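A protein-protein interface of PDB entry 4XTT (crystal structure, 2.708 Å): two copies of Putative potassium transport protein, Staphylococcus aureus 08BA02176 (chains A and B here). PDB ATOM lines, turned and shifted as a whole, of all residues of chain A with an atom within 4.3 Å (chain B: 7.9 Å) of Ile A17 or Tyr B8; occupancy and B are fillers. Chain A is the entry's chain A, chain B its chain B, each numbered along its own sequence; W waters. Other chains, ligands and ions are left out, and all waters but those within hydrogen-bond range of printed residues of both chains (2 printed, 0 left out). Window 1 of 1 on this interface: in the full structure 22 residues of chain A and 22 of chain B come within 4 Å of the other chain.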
ATOM      1  N   SER A   2      22.617 -17.417 -10.529  1.00  0.00           N
ATOM      2  CA  SER A   2      23.448 -18.518 -10.113  1.00  0.00           C
ATOM      3  C   SER A   2      24.881 -18.259 -10.553  1.00  0.00           C
ATOM      4  O   SER A   2      25.796 -18.925 -10.115  1.00  0.00           O
ATOM      5  CB  SER A   2      22.890 -19.817 -10.676  1.00  0.00           C
ATOM      6  OG  SER A   2      23.672 -20.396 -11.677  1.00  0.00           O
ATOM      7  N   VAL A   5      26.974 -15.935  -8.287  1.00  0.00           N
ATOM      8  CA  VAL A   5      27.791 -16.680  -7.342  1.00  0.00           C
ATOM      9  C   VAL A   5      29.102 -16.998  -8.024  1.00  0.00           C
ATOM     10  O   VAL A   5      30.174 -16.865  -7.442  1.00  0.00           O
ATOM     11  CB  VAL A   5      27.129 -18.001  -6.899  1.00  0.00           C
ATOM     12  CG1 VAL A   5      28.130 -18.861  -6.133  1.00  0.00           C
ATOM     13  CG2 VAL A   5      25.875 -17.729  -6.075  1.00  0.00           C
ATOM     14  N   LEU A   6      29.006 -17.402  -9.282  1.00  0.00           N
ATOM     15  CA  LEU A   6      30.185 -17.778 -10.040  1.00  0.00           C
ATOM     16  C   LEU A   6      31.012 -16.555 -10.428  1.00  0.00           C
ATOM     17  O   LEU A   6      32.237 -16.625 -10.494  1.00  0.00           O
ATOM     18  CB  LEU A   6      29.775 -18.589 -11.270  1.00  0.00           C
ATOM     19  CG  LEU A   6      30.867 -19.085 -12.215  1.00  0.00           C
ATOM     20  CD1 LEU A   6      31.979 -19.802 -11.454  1.00  0.00           C
ATOM     21  CD2 LEU A   6      30.229 -20.044 -13.202  1.00  0.00           C
ATOM     22  N   LEU A   9      33.231 -15.453  -7.384  1.00  0.00           N
ATOM     23  CA  LEU A   9      34.360 -16.357  -7.189  1.00  0.00           C
ATOM     24  C   LEU A   9      35.505 -16.115  -8.163  1.00  0.00           C
ATOM     25  O   LEU A   9      36.670 -16.330  -7.822  1.00  0.00           O
ATOM     26  CB  LEU A   9      33.887 -17.800  -7.303  1.00  0.00           C
ATOM     27  CG  LEU A   9      32.953 -18.228  -6.175  1.00  0.00           C
ATOM     28  CD1 LEU A   9      32.248 -19.492  -6.582  1.00  0.00           C
ATOM     29  CD2 LEU A   9      33.717 -18.432  -4.872  1.00  0.00           C
ATOM     30  N   SER A  16      37.078 -19.343  -3.337  1.00  0.00           N
ATOM     31  CA  SER A  16      37.169 -20.255  -4.475  1.00  0.00           C
ATOM     32  C   SER A  16      36.328 -21.517  -4.274  1.00  0.00           C
ATOM     33  O   SER A  16      36.046 -21.902  -3.140  1.00  0.00           O
ATOM     34  CB  SER A  16      38.632 -20.618  -4.748  1.00  0.00           C
ATOM     35  OG  SER A  16      39.253 -21.153  -3.598  1.00  0.00           O
ATOM     36  N   ILE A  17      35.859 -22.102  -5.377  1.00  0.00           N
ATOM     37  CA  ILE A  17      35.203 -23.407  -5.325  1.00  0.00           C
ATOM     38  C   ILE A  17      36.187 -24.504  -5.684  1.00  0.00           C
ATOM     39  O   ILE A  17      36.887 -24.438  -6.690  1.00  0.00           O
ATOM     40  CB  ILE A  17      33.992 -23.518  -6.269  1.00  0.00           C
ATOM     41  CG1 ILE A  17      32.817 -22.730  -5.719  1.00  0.00           C
ATOM     42  CG2 ILE A  17      33.501 -24.947  -6.346  1.00  0.00           C
ATOM     43  CD1 ILE A  17      31.526 -22.949  -6.498  1.00  0.00           C
ATOM     44  N   VAL A  18      36.259 -25.498  -4.814  1.00  0.00           N
ATOM     45  CA  VAL A  18      37.243 -26.551  -4.926  1.00  0.00           C
ATOM     46  C   VAL A  18      36.538 -27.888  -4.827  1.00  0.00           C
ATOM     47  O   VAL A  18      35.586 -28.050  -4.063  1.00  0.00           O
ATOM     48  CB  VAL A  18      38.326 -26.435  -3.826  1.00  0.00           C
ATOM     49  CG1 VAL A  18      39.243 -27.645  -3.840  1.00  0.00           C
ATOM     50  CG2 VAL A  18      39.126 -25.142  -4.005  1.00  0.00           C
ATOM     51  N   ILE A  45      28.193 -27.583  -1.265  1.00  0.00           N
ATOM     52  CA  ILE A  45      27.037 -27.267  -2.110  1.00  0.00           C
ATOM     53  C   ILE A  45      26.396 -28.553  -2.622  1.00  0.00           C
ATOM     54  O   ILE A  45      25.172 -28.662  -2.721  1.00  0.00           O
ATOM     55  CB  ILE A  45      27.443 -26.365  -3.302  1.00  0.00           C
ATOM     56  CG1 ILE A  45      28.135 -25.107  -2.785  1.00  0.00           C
ATOM     57  CG2 ILE A  45      26.239 -25.987  -4.134  1.00  0.00           C
ATOM     58  CD1 ILE A  45      28.675 -24.206  -3.875  1.00  0.00           C
ATOM     59  N   ILE A  70      31.907 -30.862  -3.440  1.00  0.00           N
ATOM     60  CA  ILE A  70      32.070 -29.567  -4.075  1.00  0.00           C
ATOM     61  C   ILE A  70      31.963 -28.488  -2.994  1.00  0.00           C
ATOM     62  O   ILE A  70      30.886 -28.236  -2.441  1.00  0.00           O
ATOM     63  CB  ILE A  70      31.029 -29.350  -5.183  1.00  0.00           C
ATOM     64  CG1 ILE A  70      31.013 -30.556  -6.122  1.00  0.00           C
ATOM     65  CG2 ILE A  70      31.326 -28.080  -5.947  1.00  0.00           C
ATOM     66  CD1 ILE A  70      30.036 -30.433  -7.268  1.00  0.00           C
ATOM     67  N   MET A  71      33.086 -27.844  -2.702  1.00  0.00           N
ATOM     68  CA  MET A  71      33.154 -26.973  -1.540  1.00  0.00           C
ATOM     69  C   MET A  71      33.358 -25.527  -1.934  1.00  0.00           C
ATOM     70  O   MET A  71      34.021 -25.220  -2.928  1.00  0.00           O
ATOM     71  CB  MET A  71      34.286 -27.406  -0.619  1.00  0.00           C
ATOM     72  CG  MET A  71      34.275 -28.865  -0.259  1.00  0.00           C
ATOM     73  SD  MET A  71      35.720 -29.284   0.725  1.00  0.00           S
ATOM     74  CE  MET A  71      37.005 -28.611  -0.322  1.00  0.00           C
ATOM     75  N   ILE A  72      32.813 -24.636  -1.120  1.00  0.00           N
ATOM     76  CA  ILE A  72      32.981 -23.214  -1.335  1.00  0.00           C
ATOM     77  C   ILE A  72      33.271 -22.544   0.005  1.00  0.00           C
ATOM     78  O   ILE A  72      32.623 -22.839   1.011  1.00  0.00           O
ATOM     79  CB  ILE A  72      31.732 -22.634  -2.035  1.00  0.00           C
ATOM     80  CG1 ILE A  72      31.947 -21.185  -2.444  1.00  0.00           C
ATOM     81  CG2 ILE A  72      30.492 -22.772  -1.162  1.00  0.00           C
ATOM     82  CD1 ILE A  72      30.819 -20.670  -3.304  1.00  0.00           C
ATOM     83  N   ALA B   1      40.124 -26.664 -10.546  1.00  0.00           N
ATOM     84  CA  ALA B   1      39.699 -25.266 -10.561  1.00  0.00           C
ATOM     85  C   ALA B   1      39.020 -24.904 -11.876  1.00  0.00           C
ATOM     86  O   ALA B   1      38.339 -23.888 -11.973  1.00  0.00           O
ATOM     87  CB  ALA B   1      40.879 -24.348 -10.311  1.00  0.00           C
ATOM     88  N   SER B   2      39.209 -25.740 -12.888  1.00  0.00           N
ATOM     89  CA  SER B   2      38.485 -25.586 -14.140  1.00  0.00           C
ATOM     90  C   SER B   2      37.445 -26.685 -14.314  1.00  0.00           C
ATOM     91  O   SER B   2      36.438 -26.498 -15.002  1.00  0.00           O
ATOM     92  CB  SER B   2      39.464 -25.597 -15.315  1.00  0.00           C
ATOM     93  OG  SER B   2      38.795 -25.840 -16.533  1.00  0.00           O
ATOM     94  N   ALA B   3      37.670 -27.819 -13.658  1.00  0.00           N
ATOM     95  CA  ALA B   3      36.678 -28.875 -13.635  1.00  0.00           C
ATOM     96  C   ALA B   3      35.670 -28.565 -12.537  1.00  0.00           C
ATOM     97  O   ALA B   3      34.500 -28.943 -12.597  1.00  0.00           O
ATOM     98  CB  ALA B   3      37.335 -30.215 -13.397  1.00  0.00           C
ATOM     99  N   SER B   4      36.150 -27.841 -11.538  1.00  0.00           N
ATOM    100  CA  SER B   4      35.335 -27.404 -10.422  1.00  0.00           C
ATOM    101  C   SER B   4      34.258 -26.413 -10.854  1.00  0.00           C
ATOM    102  O   SER B   4      33.137 -26.434 -10.355  1.00  0.00           O
ATOM    103  CB  SER B   4      36.243 -26.777  -9.358  1.00  0.00           C
ATOM    104  OG  SER B   4      35.649 -26.804  -8.079  1.00  0.00           O
ATOM    105  N   VAL B   5      34.596 -25.593 -11.839  1.00  0.00           N
ATOM    106  CA  VAL B   5      33.686 -24.583 -12.373  1.00  0.00           C
ATOM    107  C   VAL B   5      32.655 -25.236 -13.273  1.00  0.00           C
ATOM    108  O   VAL B   5      31.473 -24.898 -13.243  1.00  0.00           O
ATOM    109  CB  VAL B   5      34.454 -23.497 -13.179  1.00  0.00           C
ATOM    110  CG1 VAL B   5      33.500 -22.614 -13.971  1.00  0.00           C
ATOM    111  CG2 VAL B   5      35.327 -22.673 -12.261  1.00  0.00           C
ATOM    112  N   LEU B   6      33.112 -26.193 -14.070  1.00  0.00           N
ATOM    113  CA  LEU B   6      32.240 -26.851 -15.026  1.00  0.00           C
ATOM    114  C   LEU B   6      31.207 -27.740 -14.322  1.00  0.00           C
ATOM    115  O   LEU B   6      30.074 -27.878 -14.788  1.00  0.00           O
ATOM    116  CB  LEU B   6      33.096 -27.656 -16.003  1.00  0.00           C
ATOM    117  CG  LEU B   6      32.433 -28.448 -17.111  1.00  0.00           C
ATOM    118  CD1 LEU B   6      31.499 -27.550 -17.886  1.00  0.00           C
ATOM    119  CD2 LEU B   6      33.523 -28.974 -18.007  1.00  0.00           C
ATOM    120  N   ASP B   7      31.583 -28.306 -13.179  1.00  0.00           N
ATOM    121  CA  ASP B   7      30.654 -29.110 -12.395  1.00  0.00           C
ATOM    122  C   ASP B   7      29.603 -28.212 -11.767  1.00  0.00           C
ATOM    123  O   ASP B   7      28.446 -28.604 -11.625  1.00  0.00           O
ATOM    124  CB  ASP B   7      31.383 -29.919 -11.322  1.00  0.00           C
ATOM    125  CG  ASP B   7      32.045 -31.170 -11.881  1.00  0.00           C
ATOM    126  OD1 ASP B   7      31.711 -31.576 -13.013  1.00  0.00           O
ATOM    127  OD2 ASP B   7      32.895 -31.756 -11.180  1.00  0.00           O
ATOM    128  N   TYR B   8      30.006 -27.008 -11.377  1.00  0.00           N
ATOM    129  CA  TYR B   8      29.048 -26.039 -10.862  1.00  0.00           C
ATOM    130  C   TYR B   8      28.040 -25.656 -11.949  1.00  0.00           C
ATOM    131  O   TYR B   8      26.834 -25.627 -11.692  1.00  0.00           O
ATOM    132  CB  TYR B   8      29.753 -24.783 -10.356  1.00  0.00           C
ATOM    133  CG  TYR B   8      28.796 -23.682  -9.928  1.00  0.00           C
ATOM    134  CD1 TYR B   8      28.238 -23.672  -8.654  1.00  0.00           C
ATOM    135  CD2 TYR B   8      28.425 -22.674 -10.809  1.00  0.00           C
ATOM    136  CE1 TYR B   8      27.363 -22.673  -8.263  1.00  0.00           C
ATOM    137  CE2 TYR B   8      27.546 -21.676 -10.428  1.00  0.00           C
ATOM    138  CZ  TYR B   8      27.018 -21.678  -9.155  1.00  0.00           C
ATOM    139  OH  TYR B   8      26.140 -20.679  -8.781  1.00  0.00           O
ATOM    140  N   LEU B   9      28.537 -25.359 -13.156  1.00  0.00           N
ATOM    141  CA  LEU B   9      27.659 -24.963 -14.258  1.00  0.00           C
ATOM    142  C   LEU B   9      26.712 -26.095 -14.614  1.00  0.00           C
ATOM    143  O   LEU B   9      25.541 -25.862 -14.905  1.00  0.00           O
ATOM    144  CB  LEU B   9      28.449 -24.550 -15.496  1.00  0.00           C
ATOM    145  CG  LEU B   9      29.272 -23.257 -15.463  1.00  0.00           C
ATOM    146  CD1 LEU B   9      30.232 -23.216 -16.634  1.00  0.00           C
ATOM    147  CD2 LEU B   9      28.368 -22.036 -15.491  1.00  0.00           C
ATOM    148  N   GLU B  10      27.214 -27.322 -14.561  1.00  0.00           N
ATOM    149  CA  GLU B  10      26.394 -28.483 -14.859  1.00  0.00           C
ATOM    150  C   GLU B  10      25.362 -28.658 -13.759  1.00  0.00           C
ATOM    151  O   GLU B  10      24.213 -29.023 -14.012  1.00  0.00           O
ATOM    152  CB  GLU B  10      27.254 -29.738 -14.990  1.00  0.00           C
ATOM    153  CG  GLU B  10      26.476 -30.995 -15.377  1.00  0.00           C
ATOM    154  CD  GLU B  10      27.379 -32.204 -15.478  1.00  0.00           C
ATOM    155  OE1 GLU B  10      28.607 -32.037 -15.290  1.00  0.00           O
ATOM    156  OE2 GLU B  10      26.868 -33.316 -15.742  1.00  0.00           O
ATOM    157  N   LEU B  11      25.756 -28.307 -12.542  1.00  0.00           N
ATOM    158  CA  LEU B  11      24.897 -28.494 -11.385  1.00  0.00           C
ATOM    159  C   LEU B  11      23.846 -27.395 -11.296  1.00  0.00           C
ATOM    160  O   LEU B  11      22.723 -27.625 -10.837  1.00  0.00           O
ATOM    161  CB  LEU B  11      25.752 -28.502 -10.119  1.00  0.00           C
ATOM    162  CG  LEU B  11      25.139 -28.175  -8.759  1.00  0.00           C
ATOM    163  CD1 LEU B  11      24.338 -29.360  -8.247  1.00  0.00           C
ATOM    164  CD2 LEU B  11      26.237 -27.793  -7.769  1.00  0.00           C
ATOM    165  N   ALA B  12      24.186 -26.221 -11.817  1.00  0.00           N
ATOM    166  CA  ALA B  12      23.267 -25.092 -11.811  1.00  0.00           C
ATOM    167  C   ALA B  12      22.216 -25.271 -12.886  1.00  0.00           C
ATOM    168  O   ALA B  12      21.179 -24.611 -12.871  1.00  0.00           O
ATOM    169  CB  ALA B  12      24.016 -23.797 -12.018  1.00  0.00           C
ATOM    170  N   ASP B  13      22.486 -26.202 -13.796  1.00  0.00           N
ATOM    171  CA  ASP B  13      21.664 -26.397 -14.977  1.00  0.00           C
ATOM    172  C   ASP B  13      20.796 -27.647 -14.854  1.00  0.00           C
ATOM    173  O   ASP B  13      20.019 -27.962 -15.754  1.00  0.00           O
ATOM    174  CB  ASP B  13      22.570 -26.514 -16.208  1.00  0.00           C
ATOM    175  CG  ASP B  13      21.814 -26.409 -17.512  1.00  0.00           C
ATOM    176  OD1 ASP B  13      20.756 -25.741 -17.547  1.00  0.00           O
ATOM    177  OD2 ASP B  13      22.279 -27.010 -18.504  1.00  0.00           O
ATOM    178  N   GLU B  14      20.893 -28.328 -13.717  1.00  0.00           N
ATOM    179  CA  GLU B  14      20.091 -29.515 -13.483  1.00  0.00           C
ATOM    180  C   GLU B  14      19.282 -29.366 -12.202  1.00  0.00           C
ATOM    181  O   GLU B  14      18.322 -30.102 -11.969  1.00  0.00           O
ATOM    182  CB  GLU B  14      20.989 -30.753 -13.388  1.00  0.00           C
ATOM    183  CG  GLU B  14      21.576 -31.242 -14.706  1.00  0.00           C
ATOM    184  CD  GLU B  14      22.361 -32.537 -14.548  1.00  0.00           C
ATOM    185  OE1 GLU B  14      21.763 -33.548 -14.118  1.00  0.00           O
ATOM    186  OE2 GLU B  14      23.574 -32.544 -14.849  1.00  0.00           O
ATOM    187  N   HIS B  15      19.686 -28.422 -11.361  1.00  0.00           N
ATOM    188  CA  HIS B  15      18.954 -28.111 -10.140  1.00  0.00           C
ATOM    189  C   HIS B  15      18.841 -26.606 -10.067  1.00  0.00           C
ATOM    190  O   HIS B  15      19.764 -25.906 -10.479  1.00  0.00           O
ATOM    191  CB  HIS B  15      19.665 -28.713  -8.923  1.00  0.00           C
ATOM    192  CG  HIS B  15      19.940 -30.179  -9.065  1.00  0.00           C
ATOM    193  ND1 HIS B  15      21.139 -30.675  -9.537  1.00  0.00           N
ATOM    194  CD2 HIS B  15      19.151 -31.256  -8.843  1.00  0.00           C
ATOM    195  CE1 HIS B  15      21.081 -31.993  -9.578  1.00  0.00           C
ATOM    196  NE2 HIS B  15      19.888 -32.372  -9.161  1.00  0.00           N
ATOM    197  N   ILE B  17      18.924 -22.819  -8.831  1.00  0.00           N
ATOM    198  CA  ILE B  17      19.485 -21.875  -7.872  1.00  0.00           C
ATOM    199  C   ILE B  17      18.681 -20.573  -7.925  1.00  0.00           C
ATOM    200  O   ILE B  17      18.542 -19.960  -8.981  1.00  0.00           O
ATOM    201  CB  ILE B  17      20.966 -21.611  -8.160  1.00  0.00           C
ATOM    202  CG1 ILE B  17      21.757 -22.921  -8.089  1.00  0.00           C
ATOM    203  CG2 ILE B  17      21.509 -20.548  -7.226  1.00  0.00           C
ATOM    204  CD1 ILE B  17      23.249 -22.756  -8.202  1.00  0.00           C
ATOM    205  N   ILE B  45      23.730 -20.930  -0.262  1.00  0.00           N
ATOM    206  CA  ILE B  45      25.034 -20.742  -0.879  1.00  0.00           C
ATOM    207  C   ILE B  45      25.683 -19.420  -0.501  1.00  0.00           C
ATOM    208  O   ILE B  45      26.880 -19.377  -0.213  1.00  0.00           O
ATOM    209  CB  ILE B  45      24.917 -20.819  -2.420  1.00  0.00           C
ATOM    210  CG1 ILE B  45      24.287 -22.151  -2.839  1.00  0.00           C
ATOM    211  CG2 ILE B  45      26.280 -20.648  -3.087  1.00  0.00           C
ATOM    212  CD1 ILE B  45      24.018 -22.243  -4.330  1.00  0.00           C
ATOM    213  N   PHE B  53      28.772  -9.129  -1.095  1.00  0.00           N
ATOM    214  CA  PHE B  53      28.476 -10.523  -1.383  1.00  0.00           C
ATOM    215  C   PHE B  53      29.060 -11.403  -0.292  1.00  0.00           C
ATOM    216  O   PHE B  53      30.273 -11.628  -0.240  1.00  0.00           O
ATOM    217  CB  PHE B  53      29.036 -10.921  -2.747  1.00  0.00           C
ATOM    218  CG  PHE B  53      28.346 -12.104  -3.354  1.00  0.00           C
ATOM    219  CD1 PHE B  53      27.223 -11.926  -4.144  1.00  0.00           C
ATOM    220  CD2 PHE B  53      28.807 -13.391  -3.127  1.00  0.00           C
ATOM    221  CE1 PHE B  53      26.574 -13.007  -4.699  1.00  0.00           C
ATOM    222  CE2 PHE B  53      28.165 -14.474  -3.679  1.00  0.00           C
ATOM    223  CZ  PHE B  53      27.044 -14.284  -4.467  1.00  0.00           C
ATOM    224  N   ILE B  55      29.794 -14.840   0.748  1.00  0.00           N
ATOM    225  CA  ILE B  55      29.875 -16.224   0.303  1.00  0.00           C
ATOM    226  C   ILE B  55      29.970 -17.126   1.527  1.00  0.00           C
ATOM    227  O   ILE B  55      30.515 -16.719   2.556  1.00  0.00           O
ATOM    228  CB  ILE B  55      31.079 -16.453  -0.633  1.00  0.00           C
ATOM    229  CG1 ILE B  55      30.817 -17.644  -1.546  1.00  0.00           C
ATOM    230  CG2 ILE B  55      32.368 -16.646   0.146  1.00  0.00           C
ATOM    231  CD1 ILE B  55      29.625 -17.447  -2.450  1.00  0.00           C
ATOM    232  N   SER B  56      29.448 -18.344   1.408  1.00  0.00           N
ATOM    233  CA  SER B  56      29.388 -19.307   2.521  1.00  0.00           C
ATOM    234  C   SER B  56      29.075 -18.666   3.879  1.00  0.00           C
ATOM    235  O   SER B  56      29.923 -18.660   4.772  1.00  0.00           O
ATOM    236  CB  SER B  56      30.705 -20.081   2.618  1.00  0.00           C
ATOM    237  OG  SER B  56      30.791 -21.061   1.600  1.00  0.00           O
ATOM    238  N   ILE B  70      20.742 -16.695  -1.600  1.00  0.00           N
ATOM    239  CA  ILE B  70      20.901 -17.510  -2.803  1.00  0.00           C
ATOM    240  C   ILE B  70      20.840 -19.007  -2.433  1.00  0.00           C
ATOM    241  O   ILE B  70      21.651 -19.506  -1.654  1.00  0.00           O
ATOM    242  CB  ILE B  70      22.197 -17.170  -3.539  1.00  0.00           C
ATOM    243  CG1 ILE B  70      22.293 -15.656  -3.735  1.00  0.00           C
ATOM    244  CG2 ILE B  70      22.246 -17.891  -4.872  1.00  0.00           C
ATOM    245  CD1 ILE B  70      23.531 -15.202  -4.472  1.00  0.00           C
ATOM    246  N   ILE B  72      19.779 -23.364  -3.139  1.00  0.00           N
ATOM    247  CA  ILE B  72      19.736 -24.493  -4.056  1.00  0.00           C
ATOM    248  C   ILE B  72      18.958 -25.636  -3.426  1.00  0.00           C
ATOM    249  O   ILE B  72      19.106 -25.943  -2.240  1.00  0.00           O
ATOM    250  CB  ILE B  72      21.149 -24.989  -4.471  1.00  0.00           C
ATOM    251  CG1 ILE B  72      21.053 -25.980  -5.635  1.00  0.00           C
ATOM    252  CG2 ILE B  72      21.918 -25.565  -3.284  1.00  0.00           C
ATOM    253  CD1 ILE B  72      22.383 -26.353  -6.218  1.00  0.00           C
HETATM  254  O   HOH W   1      39.716 -26.247  -7.474  1.00  0.00           O
HETATM  255  O   HOH W   2      19.845 -19.015 -11.706  1.00  0.00           O
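Water W1 lies within hydrogen-bond range of N of Ala B1 (3.1 Å) and O of Ile A17 (3.4 Å). Water W2 bridges O of Ile B17 (3.2 Å) and N of Ser A2 (3.4 Å).
Along chain B the printed residues that touch a printed residue of chain A span positions 4 to 70. Among the printed residues, 14 pairs touch across the chains.
N of Met A71 sits at hydrogen-bond distance from O of Val A18 (2.9 Å). The backbone NH of Ser B56 sits at hydrogen-bond distance from the backbone carbonyl oxygen of Ile B45 (3.2 Å). The backbone carbonyl oxygen (O) of Ile B70 sits at hydrogen-bond distance from the backbone NH (N) of Ile B45 (2.9 Å).
OG of Ser A2 touches CB of Ala B12, at 3.4 Å. OH of Tyr B8 touches CB of Val A5, 3.4 Å away. Ile B45 touches Val A5 (CG2 to CG1, 3.99 Å). Phe B53 touches Val A5 (CZ to CA, 3.8 Å). CG2 of Val A5 touches CD1 of Ile B70, 3.8 Å away. Tyr B8 touches Leu A6. Leu A6 touches Leu B9 (CD2 to CD2, 3.6 Å). Tyr B8 touches Ile A17 (CD1 to CD1, 3.998 Å). Val A18 touches Ser B4 (C to OG, 3.5 Å). CD1 of Ile A72 touches CG1 of Ile B55 (3.5 Å).
Ser A2 touches Ile B17, but with the chains exchanged Ile A17 does not touch Ser B2 (6.7 Å). Val A5 touches Ile B45, but with the chains exchanged Ile A45 does not touch Val B5 (9.8 Å). Val A5 touches Ile B70, but with the chains exchanged Ile A70 does not touch Val B5 (7.2 Å). Leu A6 touches Leu B9, but with the chains exchanged Leu A9 does not touch Leu B6 (10.1 Å).
The backbone carbonyl oxygen (O) of Ile A17 sits at hydrogen-bond distance from the side-chain hydroxyl (OG) of Ser B4 (3.0 Å). O of Ile A72 sits at hydrogen-bond distance from OG of Ser B56 (2.6 Å). O of Ser A2 sits close to OH of Tyr B8, at 2.2 Å.
Of the printed residues of chain B, Ile A17 touches Ser B4 (3.0 Å) and Tyr B8 (3.998 Å). Printed residues of chain A within 4 Å of Tyr B8: Ser A2 (2.2 Å), Val A5 (3.4 Å), Leu A6 (3.9 Å) and Ile A17 (3.998 Å). Of the printed residues of chain A, Leu B9 touches Leu A6 (3.6 Å). Of the printed residues of chain B, Leu A6 touches Tyr B8 and Leu B9. Of the printed residues of chain A, Ser B56 touches Ile A72. Of the printed residues of chain A, Ile B45 touches Val A5 (3.99 Å). Printed residues of chain B within 4 Å of Val A18: Ser B4 (3.5 Å). The nearest printed residue of chain B that does not touch Ile A17 is Ala B1 (4.9 Å). The nearest printed residue of chain A that does not touch Tyr B8 is Ile A45 (4.8 Å). The nearest printed residue of chain A that does not touch Phe B53 is Leu A6 (6.1 Å).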
